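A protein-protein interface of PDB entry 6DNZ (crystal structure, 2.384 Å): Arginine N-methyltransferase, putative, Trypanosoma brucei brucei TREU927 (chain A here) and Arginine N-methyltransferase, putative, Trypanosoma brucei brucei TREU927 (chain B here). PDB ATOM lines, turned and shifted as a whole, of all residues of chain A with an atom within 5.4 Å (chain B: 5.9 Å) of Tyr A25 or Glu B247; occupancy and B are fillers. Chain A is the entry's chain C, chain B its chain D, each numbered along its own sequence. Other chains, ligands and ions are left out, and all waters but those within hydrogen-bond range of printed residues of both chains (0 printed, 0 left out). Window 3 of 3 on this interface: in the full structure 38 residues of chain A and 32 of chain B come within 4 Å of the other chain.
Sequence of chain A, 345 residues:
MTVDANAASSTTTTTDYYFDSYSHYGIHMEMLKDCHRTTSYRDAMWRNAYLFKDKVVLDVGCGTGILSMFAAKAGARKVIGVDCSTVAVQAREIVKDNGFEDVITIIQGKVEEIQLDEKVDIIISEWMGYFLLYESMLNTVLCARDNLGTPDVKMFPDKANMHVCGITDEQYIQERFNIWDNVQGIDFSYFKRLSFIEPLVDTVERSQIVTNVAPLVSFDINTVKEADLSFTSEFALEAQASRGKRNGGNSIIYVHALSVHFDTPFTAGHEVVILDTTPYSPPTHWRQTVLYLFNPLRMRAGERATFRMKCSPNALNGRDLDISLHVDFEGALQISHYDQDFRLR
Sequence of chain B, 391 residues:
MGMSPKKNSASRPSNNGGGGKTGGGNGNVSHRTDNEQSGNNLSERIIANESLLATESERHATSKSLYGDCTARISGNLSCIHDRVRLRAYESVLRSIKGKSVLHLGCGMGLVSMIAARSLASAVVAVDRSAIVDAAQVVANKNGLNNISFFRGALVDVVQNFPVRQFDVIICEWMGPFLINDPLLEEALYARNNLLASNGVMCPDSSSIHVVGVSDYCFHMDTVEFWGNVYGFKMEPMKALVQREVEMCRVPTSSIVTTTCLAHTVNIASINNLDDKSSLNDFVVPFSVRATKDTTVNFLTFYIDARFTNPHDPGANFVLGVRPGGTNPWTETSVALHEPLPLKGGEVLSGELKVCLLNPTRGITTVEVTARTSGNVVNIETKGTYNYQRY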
ATOM      1  N   SER A  23      16.409  -2.141   8.829  1.00  0.00           N
ATOM      2  CA  SER A  23      16.874  -2.329   7.461  1.00  0.00           C
ATOM      3  C   SER A  23      18.271  -2.932   7.410  1.00  0.00           C
ATOM      4  O   SER A  23      18.738  -3.282   6.321  1.00  0.00           O
ATOM      5  CB  SER A  23      16.857  -0.994   6.713  1.00  0.00           C
ATOM      6  OG  SER A  23      17.653  -0.028   7.375  1.00  0.00           O
ATOM      7  N   HIS A  24      18.934  -3.058   8.555  1.00  0.00           N
ATOM      8  CA  HIS A  24      20.261  -3.644   8.661  1.00  0.00           C
ATOM      9  C   HIS A  24      20.142  -5.091   9.125  1.00  0.00           C
ATOM     10  O   HIS A  24      19.243  -5.446   9.892  1.00  0.00           O
ATOM     11  CB  HIS A  24      21.122  -2.831   9.633  1.00  0.00           C
ATOM     12  CG  HIS A  24      22.537  -3.306   9.741  1.00  0.00           C
ATOM     13  ND1 HIS A  24      23.008  -3.996  10.838  1.00  0.00           N
ATOM     14  CD2 HIS A  24      23.589  -3.180   8.898  1.00  0.00           C
ATOM     15  CE1 HIS A  24      24.286  -4.281  10.661  1.00  0.00           C
ATOM     16  NE2 HIS A  24      24.662  -3.797   9.491  1.00  0.00           N
ATOM     17  N   TYR A  25      21.062  -5.933   8.648  1.00  0.00           N
ATOM     18  CA  TYR A  25      20.943  -7.370   8.865  1.00  0.00           C
ATOM     19  C   TYR A  25      21.243  -7.783  10.300  1.00  0.00           C
ATOM     20  O   TYR A  25      20.771  -8.838  10.736  1.00  0.00           O
ATOM     21  CB  TYR A  25      21.887  -8.121   7.925  1.00  0.00           C
ATOM     22  CG  TYR A  25      23.300  -8.237   8.450  1.00  0.00           C
ATOM     23  CD1 TYR A  25      23.712  -9.370   9.138  1.00  0.00           C
ATOM     24  CD2 TYR A  25      24.220  -7.215   8.262  1.00  0.00           C
ATOM     25  CE1 TYR A  25      24.998  -9.484   9.619  1.00  0.00           C
ATOM     26  CE2 TYR A  25      25.510  -7.320   8.743  1.00  0.00           C
ATOM     27  CZ  TYR A  25      25.894  -8.456   9.421  1.00  0.00           C
ATOM     28  OH  TYR A  25      27.176  -8.574   9.905  1.00  0.00           O
ATOM     29  N   GLY A  26      22.018  -6.985  11.038  1.00  0.00           N
ATOM     30  CA  GLY A  26      22.495  -7.425  12.340  1.00  0.00           C
ATOM     31  C   GLY A  26      21.371  -7.767  13.299  1.00  0.00           C
ATOM     32  O   GLY A  26      21.396  -8.807  13.959  1.00  0.00           O
ATOM     33  N   ILE A  27      20.371  -6.890  13.394  1.00  0.00           N
ATOM     34  CA  ILE A  27      19.306  -7.093  14.371  1.00  0.00           C
ATOM     35  C   ILE A  27      18.479  -8.320  14.015  1.00  0.00           C
ATOM     36  O   ILE A  27      18.056  -9.077  14.898  1.00  0.00           O
ATOM     37  CB  ILE A  27      18.432  -5.829  14.478  1.00  0.00           C
ATOM     38  CG1 ILE A  27      17.356  -6.007  15.553  1.00  0.00           C
ATOM     39  CG2 ILE A  27      17.776  -5.510  13.142  1.00  0.00           C
ATOM     40  CD1 ILE A  27      17.912  -6.245  16.939  1.00  0.00           C
ATOM     41  N   HIS A  28      18.226  -8.538  12.724  1.00  0.00           N
ATOM     42  CA  HIS A  28      17.445  -9.702  12.320  1.00  0.00           C
ATOM     43  C   HIS A  28      18.218 -10.994  12.539  1.00  0.00           C
ATOM     44  O   HIS A  28      17.621 -12.025  12.877  1.00  0.00           O
ATOM     45  CB  HIS A  28      17.027  -9.570  10.859  1.00  0.00           C
ATOM     46  CG  HIS A  28      16.116  -8.414  10.602  1.00  0.00           C
ATOM     47  ND1 HIS A  28      14.758  -8.476  10.823  1.00  0.00           N
ATOM     48  CD2 HIS A  28      16.371  -7.162  10.155  1.00  0.00           C
ATOM     49  CE1 HIS A  28      14.213  -7.312  10.515  1.00  0.00           C
ATOM     50  NE2 HIS A  28      15.170  -6.498  10.109  1.00  0.00           N
ATOM     51  N   MET A  29      19.530 -10.967  12.355  1.00  0.00           N
ATOM     52  CA  MET A  29      20.344 -12.143  12.606  1.00  0.00           C
ATOM     53  C   MET A  29      20.337 -12.441  14.096  1.00  0.00           C
ATOM     54  O   MET A  29      20.200 -13.590  14.506  1.00  0.00           O
ATOM     55  CB  MET A  29      21.770 -11.931  12.110  1.00  0.00           C
ATOM     56  CG  MET A  29      22.529 -13.216  11.891  1.00  0.00           C
ATOM     57  SD  MET A  29      24.378 -12.887  11.396  1.00  0.00           S
ATOM     58  CE  MET A  29      24.980 -12.045  13.050  1.00  0.00           C
ATOM     59  N   GLU A  30      20.485 -11.389  14.903  1.00  0.00           N
ATOM     60  CA  GLU A  30      20.453 -11.558  16.351  1.00  0.00           C
ATOM     61  C   GLU A  30      19.171 -12.247  16.792  1.00  0.00           C
ATOM     62  O   GLU A  30      19.200 -13.156  17.629  1.00  0.00           O
ATOM     63  CB  GLU A  30      20.592 -10.198  17.039  1.00  0.00           C
ATOM     64  CG  GLU A  30      20.540 -10.256  18.561  1.00  0.00           C
ATOM     65  CD  GLU A  30      20.679  -8.888  19.204  1.00  0.00           C
ATOM     66  OE1 GLU A  30      20.684  -7.881  18.463  1.00  0.00           O
ATOM     67  OE2 GLU A  30      20.782  -8.818  20.446  1.00  0.00           O
ATOM     68  N   PHE B 219      33.637 -17.139  10.374  1.00  0.00           N
ATOM     69  CA  PHE B 219      32.849 -15.912  10.437  1.00  0.00           C
ATOM     70  C   PHE B 219      32.029 -15.729   9.168  1.00  0.00           C
ATOM     71  O   PHE B 219      30.880 -15.277   9.222  1.00  0.00           O
ATOM     72  CB  PHE B 219      33.760 -14.708  10.668  1.00  0.00           C
ATOM     73  CG  PHE B 219      33.020 -13.412  10.867  1.00  0.00           C
ATOM     74  CD1 PHE B 219      32.523 -13.063  12.110  1.00  0.00           C
ATOM     75  CD2 PHE B 219      32.833 -12.538   9.812  1.00  0.00           C
ATOM     76  CE1 PHE B 219      31.847 -11.870  12.294  1.00  0.00           C
ATOM     77  CE2 PHE B 219      32.157 -11.345   9.991  1.00  0.00           C
ATOM     78  CZ  PHE B 219      31.665 -11.013  11.235  1.00  0.00           C
ATOM     79  N   THR B 223      27.911 -15.651   9.214  1.00  0.00           N
ATOM     80  CA  THR B 223      27.249 -14.411   8.835  1.00  0.00           C
ATOM     81  C   THR B 223      26.681 -14.433   7.430  1.00  0.00           C
ATOM     82  O   THR B 223      25.672 -13.768   7.179  1.00  0.00           O
ATOM     83  CB  THR B 223      28.221 -13.229   8.957  1.00  0.00           C
ATOM     84  OG1 THR B 223      29.378 -13.471   8.145  1.00  0.00           O
ATOM     85  CG2 THR B 223      28.660 -13.040  10.404  1.00  0.00           C
ATOM     86  N   TRP B 227      22.433 -17.506   6.367  1.00  0.00           N
ATOM     87  CA  TRP B 227      21.187 -17.205   5.676  1.00  0.00           C
ATOM     88  C   TRP B 227      20.840 -18.247   4.625  1.00  0.00           C
ATOM     89  O   TRP B 227      19.734 -18.203   4.076  1.00  0.00           O
ATOM     90  CB  TRP B 227      21.276 -15.825   5.025  1.00  0.00           C
ATOM     91  CG  TRP B 227      21.791 -14.780   5.956  1.00  0.00           C
ATOM     92  CD1 TRP B 227      23.076 -14.353   6.071  1.00  0.00           C
ATOM     93  CD2 TRP B 227      21.033 -14.037   6.918  1.00  0.00           C
ATOM     94  NE1 TRP B 227      23.169 -13.386   7.041  1.00  0.00           N
ATOM     95  CE2 TRP B 227      21.927 -13.174   7.575  1.00  0.00           C
ATOM     96  CE3 TRP B 227      19.688 -14.017   7.283  1.00  0.00           C
ATOM     97  CZ2 TRP B 227      21.519 -12.300   8.575  1.00  0.00           C
ATOM     98  CZ3 TRP B 227      19.284 -13.145   8.278  1.00  0.00           C
ATOM     99  CH2 TRP B 227      20.196 -12.301   8.912  1.00  0.00           C
ATOM    100  N   MET B 238      19.366 -11.972   2.105  1.00  0.00           N
ATOM    101  CA  MET B 238      20.053 -11.369   3.239  1.00  0.00           C
ATOM    102  C   MET B 238      21.564 -11.412   3.073  1.00  0.00           C
ATOM    103  O   MET B 238      22.265 -10.516   3.540  1.00  0.00           O
ATOM    104  CB  MET B 238      19.656 -12.075   4.533  1.00  0.00           C
ATOM    105  CG  MET B 238      18.193 -11.909   4.892  1.00  0.00           C
ATOM    106  SD  MET B 238      17.710 -10.057   5.249  1.00  0.00           S
ATOM    107  CE  MET B 238      15.793 -10.302   5.474  1.00  0.00           C
ATOM    108  N   LEU B 241      23.028  -8.185   2.011  1.00  0.00           N
ATOM    109  CA  LEU B 241      23.084  -7.174   3.061  1.00  0.00           C
ATOM    110  C   LEU B 241      24.304  -7.349   3.955  1.00  0.00           C
ATOM    111  O   LEU B 241      24.801  -6.370   4.523  1.00  0.00           O
ATOM    112  CB  LEU B 241      21.810  -7.226   3.904  1.00  0.00           C
ATOM    113  CG  LEU B 241      20.599  -6.488   3.332  1.00  0.00           C
ATOM    114  CD1 LEU B 241      20.184  -7.076   1.994  1.00  0.00           C
ATOM    115  CD2 LEU B 241      19.442  -6.525   4.322  1.00  0.00           C
ATOM    116  N   VAL B 242      24.797  -8.576   4.092  1.00  0.00           N
ATOM    117  CA  VAL B 242      25.945  -8.831   4.954  1.00  0.00           C
ATOM    118  C   VAL B 242      27.233  -8.378   4.284  1.00  0.00           C
ATOM    119  O   VAL B 242      28.048  -7.666   4.883  1.00  0.00           O
ATOM    120  CB  VAL B 242      26.012 -10.324   5.319  1.00  0.00           C
ATOM    121  CG1 VAL B 242      27.196 -10.596   6.237  1.00  0.00           C
ATOM    122  CG2 VAL B 242      24.722 -10.771   5.960  1.00  0.00           C
ATOM    123  N   GLU B 245      28.335  -4.530   3.767  1.00  0.00           N
ATOM    124  CA  GLU B 245      28.368  -3.711   4.970  1.00  0.00           C
ATOM    125  C   GLU B 245      29.756  -3.772   5.588  1.00  0.00           C
ATOM    126  O   GLU B 245      30.286  -4.861   5.832  1.00  0.00           O
ATOM    127  CB  GLU B 245      27.317  -4.184   5.978  1.00  0.00           C
ATOM    128  CG  GLU B 245      27.149  -3.263   7.176  1.00  0.00           C
ATOM    129  CD  GLU B 245      26.570  -1.911   6.799  1.00  0.00           C
ATOM    130  OE1 GLU B 245      25.643  -1.871   5.961  1.00  0.00           O
ATOM    131  OE2 GLU B 245      27.048  -0.889   7.337  1.00  0.00           O
ATOM    132  N   VAL B 246      30.345  -2.602   5.828  1.00  0.00           N
ATOM    133  CA  VAL B 246      31.601  -2.522   6.563  1.00  0.00           C
ATOM    134  C   VAL B 246      31.326  -2.872   8.018  1.00  0.00           C
ATOM    135  O   VAL B 246      30.514  -2.222   8.684  1.00  0.00           O
ATOM    136  CB  VAL B 246      32.222  -1.126   6.436  1.00  0.00           C
ATOM    137  CG1 VAL B 246      33.447  -1.007   7.324  1.00  0.00           C
ATOM    138  CG2 VAL B 246      32.580  -0.831   4.989  1.00  0.00           C
ATOM    139  N   GLU B 247      32.002  -3.901   8.517  1.00  0.00           N
ATOM    140  CA  GLU B 247      31.784  -4.392   9.870  1.00  0.00           C
ATOM    141  C   GLU B 247      32.851  -3.816  10.790  1.00  0.00           C
ATOM    142  O   GLU B 247      34.048  -4.021  10.563  1.00  0.00           O
ATOM    143  CB  GLU B 247      31.818  -5.919   9.905  1.00  0.00           C
ATOM    144  CG  GLU B 247      30.975  -6.577   8.826  1.00  0.00           C
ATOM    145  CD  GLU B 247      30.193  -7.774   9.332  1.00  0.00           C
ATOM    146  OE1 GLU B 247      29.192  -8.146   8.683  1.00  0.00           O
ATOM    147  OE2 GLU B 247      30.573  -8.341  10.378  1.00  0.00           O
ATOM    148  N   MET B 248      32.417  -3.095  11.820  1.00  0.00           N
ATOM    149  CA  MET B 248      33.326  -2.620  12.854  1.00  0.00           C
ATOM    150  C   MET B 248      33.330  -3.608  14.009  1.00  0.00           C
ATOM    151  O   MET B 248      32.349  -3.726  14.743  1.00  0.00           O
ATOM    152  CB  MET B 248      32.930  -1.232  13.349  1.00  0.00           C
ATOM    153  CG  MET B 248      33.849  -0.696  14.441  1.00  0.00           C
ATOM    154  SD  MET B 248      33.519   1.168  14.917  1.00  0.00           S
ATOM    155  CE  MET B 248      33.812   1.980  13.169  1.00  0.00           C
ATOM    156  N   CYS B 249      34.443  -4.316  14.166  1.00  0.00           N
ATOM    157  CA  CYS B 249      34.541  -5.377  15.155  1.00  0.00           C
ATOM    158  C   CYS B 249      35.999  -5.786  15.280  1.00  0.00           C
ATOM    159  O   CYS B 249      36.708  -5.871  14.275  1.00  0.00           O
ATOM    160  CB  CYS B 249      33.679  -6.579  14.754  1.00  0.00           C
ATOM    161  SG  CYS B 249      33.725  -7.944  15.925  1.00  0.00           S
ATOM    162  N   PHE B 299      38.855 -11.607   4.324  1.00  0.00           N
ATOM    163  CA  PHE B 299      38.496 -10.315   4.886  1.00  0.00           C
ATOM    164  C   PHE B 299      39.702  -9.397   4.817  1.00  0.00           C
ATOM    165  O   PHE B 299      40.843  -9.841   4.985  1.00  0.00           O
ATOM    166  CB  PHE B 299      38.037 -10.429   6.344  1.00  0.00           C
ATOM    167  CG  PHE B 299      36.693 -11.064   6.507  1.00  0.00           C
ATOM    168  CD1 PHE B 299      35.543 -10.297   6.454  1.00  0.00           C
ATOM    169  CD2 PHE B 299      36.578 -12.428   6.713  1.00  0.00           C
ATOM    170  CE1 PHE B 299      34.301 -10.876   6.600  1.00  0.00           C
ATOM    171  CE2 PHE B 299      35.338 -13.012   6.859  1.00  0.00           C
ATOM    172  CZ  PHE B 299      34.197 -12.232   6.800  1.00  0.00           C
ATOM    173  N   GLU B 332      38.911  -1.634  14.813  1.00  0.00           N
ATOM    174  CA  GLU B 332      39.122  -1.793  13.386  1.00  0.00           C
ATOM    175  C   GLU B 332      37.810  -2.108  12.677  1.00  0.00           C
ATOM    176  O   GLU B 332      36.831  -2.552  13.282  1.00  0.00           O
ATOM    177  CB  GLU B 332      40.129  -2.909  13.116  1.00  0.00           C
ATOM    178  CG  GLU B 332      39.757  -4.256  13.729  1.00  0.00           C
ATOM    179  CD  GLU B 332      40.367  -4.468  15.101  1.00  0.00           C
ATOM    180  OE1 GLU B 332      40.552  -3.475  15.837  1.00  0.00           O
ATOM    181  OE2 GLU B 332      40.676  -5.632  15.438  1.00  0.00           O
ATOM    182  N   THR B 333      37.805  -1.874  11.369  1.00  0.00           N
ATOM    183  CA  THR B 333      36.697  -2.236  10.502  1.00  0.00           C
ATOM    184  C   THR B 333      37.175  -3.279   9.498  1.00  0.00           C
ATOM    185  O   THR B 333      38.366  -3.358   9.184  1.00  0.00           O
ATOM    186  CB  THR B 333      36.144  -1.010   9.768  1.00  0.00           C
ATOM    187  OG1 THR B 333      37.187  -0.393   9.008  1.00  0.00           O
ATOM    188  CG2 THR B 333      35.587  -0.002  10.759  1.00  0.00           C
ATOM    189  N   SER B 334      36.238  -4.084   8.999  1.00  0.00           N
ATOM    190  CA  SER B 334      36.569  -5.175   8.098  1.00  0.00           C
ATOM    191  C   SER B 334      35.569  -5.231   6.954  1.00  0.00           C
ATOM    192  O   SER B 334      34.403  -4.854   7.107  1.00  0.00           O
ATOM    193  CB  SER B 334      36.586  -6.517   8.833  1.00  0.00           C
ATOM    194  OG  SER B 334      37.557  -6.510   9.862  1.00  0.00           O
ATOM    195  N   VAL B 335      36.037  -5.711   5.805  1.00  0.00           N
ATOM    196  CA  VAL B 335      35.202  -5.898   4.625  1.00  0.00           C
ATOM    197  C   VAL B 335      35.365  -7.333   4.145  1.00  0.00           C
ATOM    198  O   VAL B 335      36.481  -7.864   4.110  1.00  0.00           O
ATOM    199  CB  VAL B 335      35.560  -4.902   3.504  1.00  0.00           C
ATOM    200  CG1 VAL B 335      35.301  -3.485   3.961  1.00  0.00           C
ATOM    201  CG2 VAL B 335      37.012  -5.066   3.081  1.00  0.00           C
ATOM    202  N   ASN B 387      29.688  -0.409   2.501  1.00  0.00           N
ATOM    203  CA  ASN B 387      29.055   0.787   3.034  1.00  0.00           C
ATOM    204  C   ASN B 387      29.328   0.917   4.524  1.00  0.00           C
ATOM    205  O   ASN B 387      29.256  -0.067   5.268  1.00  0.00           O
ATOM    206  CB  ASN B 387      27.547   0.755   2.788  1.00  0.00           C
ATOM    207  CG  ASN B 387      27.203   0.589   1.325  1.00  0.00           C
ATOM    208  OD1 ASN B 387      26.609  -0.411   0.925  1.00  0.00           O
ATOM    209  ND2 ASN B 387      27.579   1.573   0.515  1.00  0.00           N
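Of the printed residues of chain A, Glu B247 touches Tyr A25. Of the printed residues of chain A, Glu B245 touches His A24. Of the printed residues of chain B, Met A29 touches Trp B227 (3.6 Å). Val B246 touches none of the printed residues of chain A. The nearest printed residue of chain A that does not touch Glu B247 is His A24 (6.3 Å).
The backbone NH (N) of Gly A26 is in hydrogen-bond range of a ring nitrogen (ND1) of His A24 (3.2 Å). NE1 of Trp B227 sits at hydrogen-bond distance from O of Thr B223, at 2.5 Å. O of Glu B247 lies within hydrogen-bond range of N of Ser B334, 2.7 Å away.
Of the 17 printed residues of chain B, 5 touch a printed residue of chain A. Printed residues of chain B that touch a printed residue of chain A: Trp B227, Leu B241, Val B242, Glu B245 and Glu B247. Hydrophobic or aromatic side chains of chain B within 4 Å of the printed part of chain A: Trp B227, Leu B241 and Val B242. Of the 8 printed residues of chain A, 4 touch a printed residue of chain B. Printed residues of chain A that touch a printed residue of chain B: Ser A23, His A24, Tyr A25 and Met A29. Hydrophobic or aromatic side chains of chain A that line the printed part of chain B: His A24, Tyr A25 and Met A29. Among the printed residues, 7 pairs touch across the chains. Among the printed residues, no Asp or Glu carboxylate lies within 4 Å of a Lys or Arg side-chain nitrogen of the other chain.
Among the printed residues, pairs that only touch across the chains: His A24 with Glu B245, Met A29 with Trp B227, Tyr A25 with Val B242, Tyr A25 with Trp B227, Ser A23 with Leu B241 and Tyr A25 with Leu B241.
The side-chain hydroxyl (OH) of Tyr A25 sits close to the side-chain carboxylate (OE2) of Glu B247.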
